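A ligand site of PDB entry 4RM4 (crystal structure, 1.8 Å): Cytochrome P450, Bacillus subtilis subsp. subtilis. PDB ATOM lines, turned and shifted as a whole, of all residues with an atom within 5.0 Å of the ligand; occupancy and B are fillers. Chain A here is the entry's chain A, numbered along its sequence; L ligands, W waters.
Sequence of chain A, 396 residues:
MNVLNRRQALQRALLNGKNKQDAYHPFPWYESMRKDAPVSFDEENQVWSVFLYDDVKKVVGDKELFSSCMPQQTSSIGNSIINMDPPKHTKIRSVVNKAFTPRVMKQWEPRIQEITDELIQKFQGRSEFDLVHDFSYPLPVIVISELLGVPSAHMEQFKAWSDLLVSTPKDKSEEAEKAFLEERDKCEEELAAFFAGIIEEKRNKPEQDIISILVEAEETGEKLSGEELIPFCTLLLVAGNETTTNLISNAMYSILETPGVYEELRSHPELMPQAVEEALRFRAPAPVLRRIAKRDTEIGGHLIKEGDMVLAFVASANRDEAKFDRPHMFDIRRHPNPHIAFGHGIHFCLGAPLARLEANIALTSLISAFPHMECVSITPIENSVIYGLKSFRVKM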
ATOM      1  N   VAL A  60     -16.399  23.464  -4.566  1.00  0.00           N
ATOM      2  CA  VAL A  60     -16.907  23.374  -3.212  1.00  0.00           C
ATOM      3  C   VAL A  60     -17.779  22.143  -3.034  1.00  0.00           C
ATOM      4  O   VAL A  60     -17.711  21.485  -2.017  1.00  0.00           O
ATOM      5  CB  VAL A  60     -17.681  24.671  -2.854  1.00  0.00           C
ATOM      6  CG1 VAL A  60     -18.517  24.504  -1.573  1.00  0.00           C
ATOM      7  CG2 VAL A  60     -16.688  25.831  -2.747  1.00  0.00           C
ATOM      8  N   SER A  68     -11.671  18.019   1.677  1.00  0.00           N
ATOM      9  CA  SER A  68     -11.710  19.063   2.700  1.00  0.00           C
ATOM     10  C   SER A  68     -10.701  18.755   3.794  1.00  0.00           C
ATOM     11  O   SER A  68     -10.550  19.528   4.752  1.00  0.00           O
ATOM     12  CB  SER A  68     -13.104  19.177   3.333  1.00  0.00           C
ATOM     13  OG  SER A  68     -14.076  19.716   2.428  1.00  0.00           O
ATOM     14  N   ILE A  81     -15.904  17.934  11.767  1.00  0.00           N
ATOM     15  CA  ILE A  81     -16.441  17.508  10.475  1.00  0.00           C
ATOM     16  C   ILE A  81     -16.076  18.397   9.270  1.00  0.00           C
ATOM     17  O   ILE A  81     -16.060  17.931   8.139  1.00  0.00           O
ATOM     18  CB  ILE A  81     -17.995  17.345  10.509  1.00  0.00           C
ATOM     19  CG1 ILE A  81     -18.681  18.605  11.034  1.00  0.00           C
ATOM     20  CG2 ILE A  81     -18.380  16.123  11.343  1.00  0.00           C
ATOM     21  CD1 ILE A  81     -20.204  18.528  10.942  1.00  0.00           C
ATOM     22  N   ILE A  82     -15.780  19.666   9.522  1.00  0.00           N
ATOM     23  CA  ILE A  82     -15.529  20.611   8.437  1.00  0.00           C
ATOM     24  C   ILE A  82     -14.259  20.228   7.681  1.00  0.00           C
ATOM     25  O   ILE A  82     -14.082  20.626   6.537  1.00  0.00           O
ATOM     26  CB  ILE A  82     -15.469  22.068   8.921  1.00  0.00           C
ATOM     27  CG1 ILE A  82     -15.659  23.023   7.743  1.00  0.00           C
ATOM     28  CG2 ILE A  82     -14.170  22.327   9.671  1.00  0.00           C
ATOM     29  CD1 ILE A  82     -16.087  24.404   8.189  1.00  0.00           C
ATOM     30  N   HIS A  89     -16.972  11.691   7.600  1.00  0.00           N
ATOM     31  CA  HIS A  89     -17.826  12.873   7.653  1.00  0.00           C
ATOM     32  C   HIS A  89     -19.298  12.491   7.657  1.00  0.00           C
ATOM     33  O   HIS A  89     -20.103  13.066   8.384  1.00  0.00           O
ATOM     34  CB  HIS A  89     -17.548  13.817   6.489  1.00  0.00           C
ATOM     35  CG  HIS A  89     -18.546  14.924   6.378  1.00  0.00           C
ATOM     36  ND1 HIS A  89     -19.695  14.833   5.624  1.00  0.00           N
ATOM     37  CD2 HIS A  89     -18.562  16.174   6.925  1.00  0.00           C
ATOM     38  CE1 HIS A  89     -20.379  15.964   5.723  1.00  0.00           C
ATOM     39  NE2 HIS A  89     -19.716  16.791   6.511  1.00  0.00           N
ATOM     40  N   ARG A  93     -21.832  13.761  10.516  1.00  0.00           N
ATOM     41  CA  ARG A  93     -22.822  14.743  10.042  1.00  0.00           C
ATOM     42  C   ARG A  93     -24.239  14.229  10.281  1.00  0.00           C
ATOM     43  O   ARG A  93     -25.088  14.959  10.762  1.00  0.00           O
ATOM     44  CB  ARG A  93     -22.619  15.087   8.558  1.00  0.00           C
ATOM     45  CG  ARG A  93     -23.610  16.105   7.967  1.00  0.00           C
ATOM     46  CD  ARG A  93     -23.560  17.469   8.669  1.00  0.00           C
ATOM     47  NE  ARG A  93     -24.654  18.343   8.240  1.00  0.00           N
ATOM     48  CZ  ARG A  93     -24.505  19.424   7.482  1.00  0.00           C
ATOM     49  NH1 ARG A  93     -23.296  19.812   7.101  1.00  0.00           N
ATOM     50  NH2 ARG A  93     -25.565  20.155   7.145  1.00  0.00           N
ATOM     51  N   PHE A 100     -30.020  20.574  14.856  1.00  0.00           N
ATOM     52  CA  PHE A 100     -30.405  21.790  14.111  1.00  0.00           C
ATOM     53  C   PHE A 100     -31.720  21.696  13.314  1.00  0.00           C
ATOM     54  O   PHE A 100     -31.964  22.506  12.412  1.00  0.00           O
ATOM     55  CB  PHE A 100     -29.236  22.228  13.209  1.00  0.00           C
ATOM     56  CG  PHE A 100     -28.071  22.741  13.993  1.00  0.00           C
ATOM     57  CD1 PHE A 100     -27.110  21.854  14.491  1.00  0.00           C
ATOM     58  CD2 PHE A 100     -27.963  24.083  14.295  1.00  0.00           C
ATOM     59  CE1 PHE A 100     -26.045  22.325  15.264  1.00  0.00           C
ATOM     60  CE2 PHE A 100     -26.902  24.560  15.061  1.00  0.00           C
ATOM     61  CZ  PHE A 100     -25.952  23.677  15.538  1.00  0.00           C
ATOM     62  N   ILE A 144     -25.029  30.808  21.586  1.00  0.00           N
ATOM     63  CA  ILE A 144     -24.443  29.476  21.473  1.00  0.00           C
ATOM     64  C   ILE A 144     -24.113  28.901  22.855  1.00  0.00           C
ATOM     65  O   ILE A 144     -24.167  27.677  23.079  1.00  0.00           O
ATOM     66  CB  ILE A 144     -23.189  29.468  20.573  1.00  0.00           C
ATOM     67  CG1 ILE A 144     -22.898  28.053  20.080  1.00  0.00           C
ATOM     68  CG2 ILE A 144     -21.986  30.090  21.284  1.00  0.00           C
ATOM     69  CD1 ILE A 144     -24.002  27.480  19.168  1.00  0.00           C
ATOM     70  N   PHE A 232     -16.533  18.686  18.062  1.00  0.00           N
ATOM     71  CA  PHE A 232     -17.727  19.234  17.420  1.00  0.00           C
ATOM     72  C   PHE A 232     -18.265  20.512  18.139  1.00  0.00           C
ATOM     73  O   PHE A 232     -18.614  21.495  17.497  1.00  0.00           O
ATOM     74  CB  PHE A 232     -18.842  18.178  17.302  1.00  0.00           C
ATOM     75  CG  PHE A 232     -20.125  18.732  16.760  1.00  0.00           C
ATOM     76  CD1 PHE A 232     -20.245  19.052  15.415  1.00  0.00           C
ATOM     77  CD2 PHE A 232     -21.207  18.981  17.601  1.00  0.00           C
ATOM     78  CE1 PHE A 232     -21.423  19.593  14.914  1.00  0.00           C
ATOM     79  CE2 PHE A 232     -22.393  19.517  17.100  1.00  0.00           C
ATOM     80  CZ  PHE A 232     -22.503  19.818  15.760  1.00  0.00           C
ATOM     81  N   LEU A 235     -16.029  23.400  17.355  1.00  0.00           N
ATOM     82  CA  LEU A 235     -16.269  23.845  15.972  1.00  0.00           C
ATOM     83  C   LEU A 235     -17.452  24.805  15.887  1.00  0.00           C
ATOM     84  O   LEU A 235     -17.418  25.763  15.115  1.00  0.00           O
ATOM     85  CB  LEU A 235     -16.497  22.652  15.047  1.00  0.00           C
ATOM     86  CG  LEU A 235     -16.756  22.993  13.575  1.00  0.00           C
ATOM     87  CD1 LEU A 235     -15.638  23.880  13.020  1.00  0.00           C
ATOM     88  CD2 LEU A 235     -16.927  21.720  12.769  1.00  0.00           C
ATOM     89  N   LEU A 236     -18.494  24.551  16.674  1.00  0.00           N
ATOM     90  CA  LEU A 236     -19.655  25.419  16.650  1.00  0.00           C
ATOM     91  C   LEU A 236     -19.289  26.868  16.985  1.00  0.00           C
ATOM     92  O   LEU A 236     -19.835  27.790  16.406  1.00  0.00           O
ATOM     93  CB  LEU A 236     -20.741  24.924  17.603  1.00  0.00           C
ATOM     94  CG  LEU A 236     -21.309  23.537  17.266  1.00  0.00           C
ATOM     95  CD1 LEU A 236     -22.513  23.272  18.187  1.00  0.00           C
ATOM     96  CD2 LEU A 236     -21.694  23.402  15.793  1.00  0.00           C
ATOM     97  N   ALA A 239     -16.856  28.029  13.939  1.00  0.00           N
ATOM     98  CA  ALA A 239     -17.592  28.177  12.672  1.00  0.00           C
ATOM     99  C   ALA A 239     -18.718  29.208  12.729  1.00  0.00           C
ATOM    100  O   ALA A 239     -19.078  29.800  11.711  1.00  0.00           O
ATOM    101  CB  ALA A 239     -18.149  26.823  12.240  1.00  0.00           C
ATOM    102  N   GLY A 240     -19.261  29.421  13.931  1.00  0.00           N
ATOM    103  CA  GLY A 240     -20.510  30.136  14.082  1.00  0.00           C
ATOM    104  C   GLY A 240     -20.472  31.506  14.749  1.00  0.00           C
ATOM    105  O   GLY A 240     -21.310  32.347  14.467  1.00  0.00           O
ATOM    106  N   THR A 243     -18.761  34.489  12.281  1.00  0.00           N
ATOM    107  CA  THR A 243     -19.494  34.568  10.999  1.00  0.00           C
ATOM    108  C   THR A 243     -20.876  35.185  11.189  1.00  0.00           C
ATOM    109  O   THR A 243     -21.342  35.982  10.370  1.00  0.00           O
ATOM    110  CB  THR A 243     -19.707  33.182  10.373  1.00  0.00           C
ATOM    111  OG1 THR A 243     -20.291  32.307  11.344  1.00  0.00           O
ATOM    112  CG2 THR A 243     -18.399  32.593   9.859  1.00  0.00           C
ATOM    113  N   THR A 244     -21.543  34.762  12.258  1.00  0.00           N
ATOM    114  CA  THR A 244     -22.870  35.283  12.566  1.00  0.00           C
ATOM    115  C   THR A 244     -22.825  36.758  12.952  1.00  0.00           C
ATOM    116  O   THR A 244     -23.683  37.547  12.529  1.00  0.00           O
ATOM    117  CB  THR A 244     -23.547  34.442  13.653  1.00  0.00           C
ATOM    118  OG1 THR A 244     -23.557  33.077  13.229  1.00  0.00           O
ATOM    119  CG2 THR A 244     -24.962  34.905  13.848  1.00  0.00           C
ATOM    120  N   LEU A 247     -22.251  38.542   9.718  1.00  0.00           N
ATOM    121  CA  LEU A 247     -23.480  38.566   8.913  1.00  0.00           C
ATOM    122  C   LEU A 247     -24.369  39.702   9.388  1.00  0.00           C
ATOM    123  O   LEU A 247     -24.872  40.500   8.590  1.00  0.00           O
ATOM    124  CB  LEU A 247     -24.247  37.232   8.987  1.00  0.00           C
ATOM    125  CG  LEU A 247     -25.670  37.239   8.372  1.00  0.00           C
ATOM    126  CD1 LEU A 247     -25.652  37.738   6.932  1.00  0.00           C
ATOM    127  CD2 LEU A 247     -26.313  35.839   8.468  1.00  0.00           C
ATOM    128  N   LEU A 280     -26.561  37.751   2.748  1.00  0.00           N
ATOM    129  CA  LEU A 280     -25.641  36.609   2.565  1.00  0.00           C
ATOM    130  C   LEU A 280     -25.013  36.644   1.184  1.00  0.00           C
ATOM    131  O   LEU A 280     -23.819  36.404   1.048  1.00  0.00           O
ATOM    132  CB  LEU A 280     -26.373  35.278   2.782  1.00  0.00           C
ATOM    133  CG  LEU A 280     -26.617  34.992   4.272  1.00  0.00           C
ATOM    134  CD1 LEU A 280     -27.831  34.092   4.470  1.00  0.00           C
ATOM    135  CD2 LEU A 280     -25.386  34.412   4.953  1.00  0.00           C
ATOM    136  N   PRO A 285     -19.894  36.564   5.011  1.00  0.00           N
ATOM    137  CA  PRO A 285     -18.890  36.683   6.073  1.00  0.00           C
ATOM    138  C   PRO A 285     -17.688  35.742   5.855  1.00  0.00           C
ATOM    139  O   PRO A 285     -16.596  36.015   6.350  1.00  0.00           O
ATOM    140  CB  PRO A 285     -19.649  36.239   7.338  1.00  0.00           C
ATOM    141  CG  PRO A 285     -21.087  36.204   6.967  1.00  0.00           C
ATOM    142  CD  PRO A 285     -21.141  35.954   5.496  1.00  0.00           C
ATOM    143  N   ALA A 286     -17.913  34.647   5.146  1.00  0.00           N
ATOM    144  CA  ALA A 286     -16.828  33.696   4.898  1.00  0.00           C
ATOM    145  C   ALA A 286     -16.548  33.631   3.412  1.00  0.00           C
ATOM    146  O   ALA A 286     -17.097  32.791   2.709  1.00  0.00           O
ATOM    147  CB  ALA A 286     -17.192  32.312   5.466  1.00  0.00           C
ATOM    148  N   LEU A 289     -13.123  29.449   0.577  1.00  0.00           N
ATOM    149  CA  LEU A 289     -13.133  28.102   1.129  1.00  0.00           C
ATOM    150  C   LEU A 289     -12.009  27.320   0.451  1.00  0.00           C
ATOM    151  O   LEU A 289     -11.723  27.555  -0.724  1.00  0.00           O
ATOM    152  CB  LEU A 289     -14.492  27.448   0.855  1.00  0.00           C
ATOM    153  CG  LEU A 289     -15.752  28.045   1.463  1.00  0.00           C
ATOM    154  CD1 LEU A 289     -16.980  27.249   0.982  1.00  0.00           C
ATOM    155  CD2 LEU A 289     -15.700  28.031   2.990  1.00  0.00           C
ATOM    156  N   ARG A 291     -10.000  23.721  -0.740  1.00  0.00           N
ATOM    157  CA  ARG A 291     -10.069  22.306  -1.063  1.00  0.00           C
ATOM    158  C   ARG A 291      -8.715  21.819  -1.552  1.00  0.00           C
ATOM    159  O   ARG A 291      -7.847  22.604  -1.934  1.00  0.00           O
ATOM    160  CB  ARG A 291     -11.139  22.033  -2.135  1.00  0.00           C
ATOM    161  CG  ARG A 291     -12.576  22.408  -1.744  1.00  0.00           C
ATOM    162  CD  ARG A 291     -13.119  21.406  -0.744  1.00  0.00           C
ATOM    163  NE  ARG A 291     -14.557  21.538  -0.493  1.00  0.00           N
ATOM    164  CZ  ARG A 291     -15.085  22.317   0.443  1.00  0.00           C
ATOM    165  NH1 ARG A 291     -14.294  23.053   1.208  1.00  0.00           N
ATOM    166  NH2 ARG A 291     -16.403  22.359   0.614  1.00  0.00           N
ATOM    167  N   ILE A 340     -24.018  31.092  -2.526  1.00  0.00           N
ATOM    168  CA  ILE A 340     -23.342  29.999  -1.873  1.00  0.00           C
ATOM    169  C   ILE A 340     -22.622  30.468  -0.611  1.00  0.00           C
ATOM    170  O   ILE A 340     -21.558  29.989  -0.268  1.00  0.00           O
ATOM    171  CB  ILE A 340     -22.462  29.199  -2.838  1.00  0.00           C
ATOM    172  CG1 ILE A 340     -21.734  30.105  -3.833  1.00  0.00           C
ATOM    173  CG2 ILE A 340     -23.332  28.251  -3.654  1.00  0.00           C
ATOM    174  CD1 ILE A 340     -21.042  29.310  -4.934  1.00  0.00           C
ATOM    175  N   ALA A 341     -23.254  31.383   0.118  1.00  0.00           N
ATOM    176  CA  ALA A 341     -22.627  31.906   1.329  1.00  0.00           C
ATOM    177  C   ALA A 341     -22.439  30.818   2.379  1.00  0.00           C
ATOM    178  O   ALA A 341     -21.520  30.909   3.202  1.00  0.00           O
ATOM    179  CB  ALA A 341     -23.441  33.039   1.889  1.00  0.00           C
ATOM    180  N   PHE A 342     -23.297  29.801   2.345  1.00  0.00           N
ATOM    181  CA  PHE A 342     -23.254  28.716   3.330  1.00  0.00           C
ATOM    182  C   PHE A 342     -22.562  27.473   2.744  1.00  0.00           C
ATOM    183  O   PHE A 342     -22.598  26.387   3.345  1.00  0.00           O
ATOM    184  CB  PHE A 342     -24.675  28.339   3.769  1.00  0.00           C
ATOM    185  CG  PHE A 342     -25.327  29.333   4.706  1.00  0.00           C
ATOM    186  CD1 PHE A 342     -26.611  29.792   4.452  1.00  0.00           C
ATOM    187  CD2 PHE A 342     -24.686  29.749   5.855  1.00  0.00           C
ATOM    188  CE1 PHE A 342     -27.236  30.654   5.339  1.00  0.00           C
ATOM    189  CE2 PHE A 342     -25.305  30.621   6.750  1.00  0.00           C
ATOM    190  CZ  PHE A 342     -26.577  31.080   6.475  1.00  0.00           C
ATOM    191  N   GLY A 343     -21.965  27.630   1.575  1.00  0.00           N
ATOM    192  CA  GLY A 343     -21.370  26.500   0.879  1.00  0.00           C
ATOM    193  C   GLY A 343     -22.370  25.746  -0.002  1.00  0.00           C
ATOM    194  O   GLY A 343     -23.401  26.299  -0.422  1.00  0.00           O
ATOM    195  N   ILE A 346     -22.033  18.326   0.730  1.00  0.00           N
ATOM    196  CA  ILE A 346     -22.020  17.613   1.997  1.00  0.00           C
ATOM    197  C   ILE A 346     -21.636  18.474   3.201  1.00  0.00           C
ATOM    198  O   ILE A 346     -22.099  18.218   4.302  1.00  0.00           O
ATOM    199  CB  ILE A 346     -21.155  16.321   1.975  1.00  0.00           C
ATOM    200  CG1 ILE A 346     -19.677  16.614   1.698  1.00  0.00           C
ATOM    201  CG2 ILE A 346     -21.740  15.299   0.995  1.00  0.00           C
ATOM    202  CD1 ILE A 346     -18.761  15.406   1.977  1.00  0.00           C
ATOM    203  N   HIS A 347     -20.801  19.498   2.986  1.00  0.00           N
ATOM    204  CA  HIS A 347     -20.350  20.350   4.082  1.00  0.00           C
ATOM    205  C   HIS A 347     -21.203  21.624   4.252  1.00  0.00           C
ATOM    206  O   HIS A 347     -20.850  22.504   5.052  1.00  0.00           O
ATOM    207  CB  HIS A 347     -18.877  20.752   3.882  1.00  0.00           C
ATOM    208  CG  HIS A 347     -17.916  19.609   3.990  1.00  0.00           C
ATOM    209  ND1 HIS A 347     -17.539  19.069   5.213  1.00  0.00           N
ATOM    210  CD2 HIS A 347     -17.238  18.910   3.049  1.00  0.00           C
ATOM    211  CE1 HIS A 347     -16.676  18.083   5.010  1.00  0.00           C
ATOM    212  NE2 HIS A 347     -16.483  17.970   3.704  1.00  0.00           N
ATOM    213  N   PHE A 348     -22.311  21.713   3.519  1.00  0.00           N
ATOM    214  CA  PHE A 348     -23.198  22.868   3.590  1.00  0.00           C
ATOM    215  C   PHE A 348     -23.491  23.201   5.047  1.00  0.00           C
ATOM    216  O   PHE A 348     -23.848  22.320   5.833  1.00  0.00           O
ATOM    217  CB  PHE A 348     -24.527  22.599   2.860  1.00  0.00           C
ATOM    218  CG  PHE A 348     -25.477  23.746   2.923  1.00  0.00           C
ATOM    219  CD1 PHE A 348     -25.444  24.749   1.950  1.00  0.00           C
ATOM    220  CD2 PHE A 348     -26.400  23.842   3.940  1.00  0.00           C
ATOM    221  CE1 PHE A 348     -26.312  25.825   2.020  1.00  0.00           C
ATOM    222  CE2 PHE A 348     -27.271  24.900   4.023  1.00  0.00           C
ATOM    223  CZ  PHE A 348     -27.238  25.903   3.050  1.00  0.00           C
ATOM    224  N   CYS A 349     -23.329  24.479   5.378  1.00  0.00           N
ATOM    225  CA  CYS A 349     -23.313  24.943   6.757  1.00  0.00           C
ATOM    226  C   CYS A 349     -24.364  24.280   7.650  1.00  0.00           C
ATOM    227  O   CYS A 349     -25.551  24.479   7.454  1.00  0.00           O
ATOM    228  CB  CYS A 349     -23.518  26.460   6.799  1.00  0.00           C
ATOM    229  SG  CYS A 349     -23.530  27.116   8.498  1.00  0.00           S
ATOM    230  N   LEU A 350     -23.909  23.509   8.628  1.00  0.00           N
ATOM    231  CA  LEU A 350     -24.836  22.902   9.598  1.00  0.00           C
ATOM    232  C   LEU A 350     -25.628  23.970  10.357  1.00  0.00           C
ATOM    233  O   LEU A 350     -26.784  23.765  10.723  1.00  0.00           O
ATOM    234  CB  LEU A 350     -24.072  22.037  10.581  1.00  0.00           C
ATOM    235  CG  LEU A 350     -24.917  21.448  11.717  1.00  0.00           C
ATOM    236  CD1 LEU A 350     -25.917  20.390  11.209  1.00  0.00           C
ATOM    237  CD2 LEU A 350     -24.035  20.867  12.795  1.00  0.00           C
ATOM    238  N   GLY A 351     -25.001  25.128  10.569  1.00  0.00           N
ATOM    239  CA  GLY A 351     -25.632  26.164  11.369  1.00  0.00           C
ATOM    240  C   GLY A 351     -26.530  27.091  10.584  1.00  0.00           C
ATOM    241  O   GLY A 351     -27.075  28.056  11.119  1.00  0.00           O
ATOM    242  N   LEU A 354     -29.710  28.255  12.135  1.00  0.00           N
ATOM    243  CA  LEU A 354     -29.492  29.044  13.344  1.00  0.00           C
ATOM    244  C   LEU A 354     -28.988  30.439  12.984  1.00  0.00           C
ATOM    245  O   LEU A 354     -29.366  31.443  13.603  1.00  0.00           O
ATOM    246  CB  LEU A 354     -28.499  28.354  14.262  1.00  0.00           C
ATOM    247  CG  LEU A 354     -28.042  29.110  15.532  1.00  0.00           C
ATOM    248  CD1 LEU A 354     -29.237  29.531  16.384  1.00  0.00           C
ATOM    249  CD2 LEU A 354     -27.049  28.277  16.356  1.00  0.00           C
ATOM    250  N   ALA A 355     -28.111  30.517  11.978  1.00  0.00           N
ATOM    251  CA  ALA A 355     -27.603  31.826  11.538  1.00  0.00           C
ATOM    252  C   ALA A 355     -28.740  32.649  10.933  1.00  0.00           C
ATOM    253  O   ALA A 355     -28.881  33.842  11.231  1.00  0.00           O
ATOM    254  CB  ALA A 355     -26.454  31.662  10.535  1.00  0.00           C
ATOM    255  N   GLU A 358     -30.910  33.722  13.957  1.00  0.00           N
ATOM    256  CA  GLU A 358     -30.254  34.809  14.688  1.00  0.00           C
ATOM    257  C   GLU A 358     -30.309  36.152  13.929  1.00  0.00           C
ATOM    258  O   GLU A 358     -30.625  37.192  14.509  1.00  0.00           O
ATOM    259  CB  GLU A 358     -28.814  34.431  15.029  1.00  0.00           C
ATOM    260  CG  GLU A 358     -28.709  33.289  16.030  1.00  0.00           C
ATOM    261  CD  GLU A 358     -27.310  33.138  16.594  1.00  0.00           C
ATOM    262  OE1 GLU A 358     -26.769  32.013  16.575  1.00  0.00           O
ATOM    263  OE2 GLU A 358     -26.715  34.161  17.019  1.00  0.00           O
HETATM  264  C1  LIG L   1     -19.887  24.940   7.437  1.00  0.00           C
HETATM  265  C2  LIG L   1     -20.656  29.613   6.472  1.00  0.00           C
HETATM  266  C3  LIG L   1     -22.790  30.181  10.822  1.00  0.00           C
HETATM  267  C4  LIG L   1     -21.569  25.636  11.994  1.00  0.00           C
HETATM  268  C5  LIG L   1     -19.947  26.151   6.771  1.00  0.00           C
HETATM  269  C6  LIG L   1     -19.563  26.394   5.397  1.00  0.00           C
HETATM  270  C7  LIG L   1     -19.776  27.682   5.130  1.00  0.00           C
HETATM  271  C8  LIG L   1     -20.315  28.300   6.318  1.00  0.00           C
HETATM  272  C9  LIG L   1     -19.500  28.412   3.780  1.00  0.00           C
HETATM  273  C10 LIG L   1     -19.014  25.345   4.390  1.00  0.00           C
HETATM  274  C11 LIG L   1     -17.542  25.091   4.631  1.00  0.00           C
HETATM  275  C12 LIG L   1     -16.913  24.313   3.504  1.00  0.00           C
HETATM  276  O1  LIG L   1     -15.674  24.116   3.565  1.00  0.00           O
HETATM  277  O2  LIG L   1     -17.640  23.886   2.559  1.00  0.00           O
HETATM  278  C13 LIG L   1     -21.332  30.139   7.551  1.00  0.00           C
HETATM  279  C14 LIG L   1     -21.912  31.465   7.606  1.00  0.00           C
HETATM  280  C15 LIG L   1     -22.483  31.623   8.809  1.00  0.00           C
HETATM  281  C16 LIG L   1     -22.306  30.394   9.552  1.00  0.00           C
HETATM  282  C17 LIG L   1     -21.854  32.484   6.450  1.00  0.00           C
HETATM  283  C18 LIG L   1     -23.264  32.820   9.390  1.00  0.00           C
HETATM  284  C19 LIG L   1     -23.793  33.735   8.577  1.00  0.00           C
HETATM  285  C20 LIG L   1     -22.674  28.991  11.498  1.00  0.00           C
HETATM  286  C21 LIG L   1     -23.227  28.690  12.801  1.00  0.00           C
HETATM  287  C22 LIG L   1     -22.888  27.440  13.108  1.00  0.00           C
HETATM  288  C23 LIG L   1     -22.110  26.913  12.023  1.00  0.00           C
HETATM  289  C24 LIG L   1     -24.068  29.693  13.624  1.00  0.00           C
HETATM  290  C25 LIG L   1     -23.181  26.598  14.375  1.00  0.00           C
HETATM  291  C26 LIG L   1     -23.657  27.101  15.516  1.00  0.00           C
HETATM  292  C27 LIG L   1     -20.989  25.037  10.900  1.00  0.00           C
HETATM  293  C28 LIG L   1     -20.464  23.701  10.893  1.00  0.00           C
HETATM  294  C29 LIG L   1     -19.934  23.472   9.477  1.00  0.00           C
HETATM  295  C30 LIG L   1     -20.202  24.699   8.761  1.00  0.00           C
HETATM  296  C31 LIG L   1     -20.454  22.721  12.089  1.00  0.00           C
HETATM  297  C32 LIG L   1     -19.276  22.182   8.934  1.00  0.00           C
HETATM  298  C33 LIG L   1     -20.380  21.313   8.325  1.00  0.00           C
HETATM  299  C34 LIG L   1     -19.781  20.084   7.676  1.00  0.00           C
HETATM  300  O3  LIG L   1     -20.542  19.126   7.406  1.00  0.00           O
HETATM  301  O4  LIG L   1     -18.536  20.078   7.473  1.00  0.00           O
HETATM  302  N1  LIG L   1     -20.395  27.344   7.303  1.00  0.00           N
HETATM  303  N2  LIG L   1     -21.582  29.526   8.764  1.00  0.00           N
HETATM  304  N3  LIG L   1     -21.991  27.881  11.047  1.00  0.00           N
HETATM  305  N4  LIG L   1     -20.827  25.586   9.630  1.00  0.00           N
HETATM  306 FE1  LIG L   1     -21.325  27.536   9.120  1.00  0.00          FE
HETATM  307  O   HOH W   1     -14.848  21.436   4.175  1.00  0.00           O
HETATM  308  O   HOH W   2     -19.948  23.286   1.463  1.00  0.00           O
HETATM  309  O   HOH W   3     -19.120  28.399   9.661  1.00  0.00           O
HETATM  310  O   HOH W   4     -14.035  25.394   5.244  1.00  0.00           O
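An oxygen (O4) of the ligand sits close to the backbone carbonyl oxygen (O) of Ile 81, 3.3 Å away.
Ile 144 touches the ligand.
CD2 of Leu 235 touches C31 of the ligand (3.7 Å).
CD2 of Leu 236 touches C25 of the ligand, 3.8 Å away.
Ala 239 touches the ligand.
Gly 240 touches the ligand (CA to C21, 3.3 Å).
Thr 243 touches the ligand.
Thr 244 touches the ligand (OG1 to C24, 3.4 Å).
Leu 247 touches the ligand (CD2 to C19, 3.3 Å).
CD of Pro 285 touches C17 of the ligand, at 3.7 Å.
Leu 289 touches the ligand (CD1 to O2, 3.8 Å).
Ala 341 touches the ligand (O to C9, 3.3 Å).
Phe 342 touches the ligand.
Gly 343 touches the ligand (N to C9, 3.4 Å).
O of Ile 346 touches O3 of the ligand, at 3.6 Å.
Leu 350 touches the ligand (N to N4, 3.8 Å).
CA of Gly 351 touches C22 of the ligand, at 3.5 Å.
CD2 of Leu 354 touches C26 of the ligand, 3.7 Å away.
Ala 355 touches the ligand (CB to C18, 3.6 Å).
Hydrophobic or aromatic side chains within 4 Å of the ligand: Ile 81, Ile 82, His 89, Ile 144, Leu 235, Leu 236, Ala 239, Leu 247, Pro 285, Leu 289, Phe 342, His 347, Leu 350, Leu 354 and Ala 355.
Within 4 Å of the ligand: Ile 81, Ile 82, His 89, Arg 93, Ile 144, Leu 235, Leu 236, Ala 239, Gly 240, Thr 243, Thr 244, Leu 247, Pro 285, Leu 289, Arg 291, Ala 341, Phe 342, Gly 343, Ile 346, His 347, Cys 349, Leu 350, Gly 351, Leu 354 and Ala 355.
The nearest printed residue that does not touch the ligand is Leu 280 (4.02 Å).
The backbone carbonyl oxygen of Val 60 is in hydrogen-bond range of the guanidinium group of Arg 291.
OG1 of Thr 243 is in hydrogen-bond range of O of Ala 239 (2.8 Å).
OG1 of Thr 243 is in hydrogen-bond range of O of Gly 240 (3.3 Å).
NH1 of Arg 93 sits at hydrogen-bond distance from O of Phe 348, 2.9 Å away.
A ring nitrogen (ND1) of His 347 lies close to the backbone carbonyl oxygen (O) of Ile 81.
The guanidinium group (NH1) of Arg 93 is in hydrogen-bond range of the backbone carbonyl oxygen (O) of Ile 346.
The guanidinium group of Arg 291 lies close to the side-chain hydroxyl of Ser 68.
N of Cys 349 is in hydrogen-bond range of O of Phe 342 (2.9 Å).
An oxygen (O3) of the ligand lies within salt-bridge range of the guanidinium group of Arg 93.
O3 of the ligand lies within hydrogen-bond range of NE2 of His 89.
The guanidinium group (NH2) of Arg 291 is in salt-bridge range of an oxygen (O2) of the ligand.
FE1 of the ligand is bound by SG of Cys 349.
The backbone NH (N) of Ile 82 lies close to an oxygen (O4) of the ligand (3.5 Å).
A ring nitrogen (ND1) of His 347 is in hydrogen-bond range of an oxygen (O4) of the ligand (2.7 Å).
Water W1 lies within hydrogen-bond range of OG of Ser 68, O of Ile 82, O1 of the ligand and NH1 of Arg 291.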
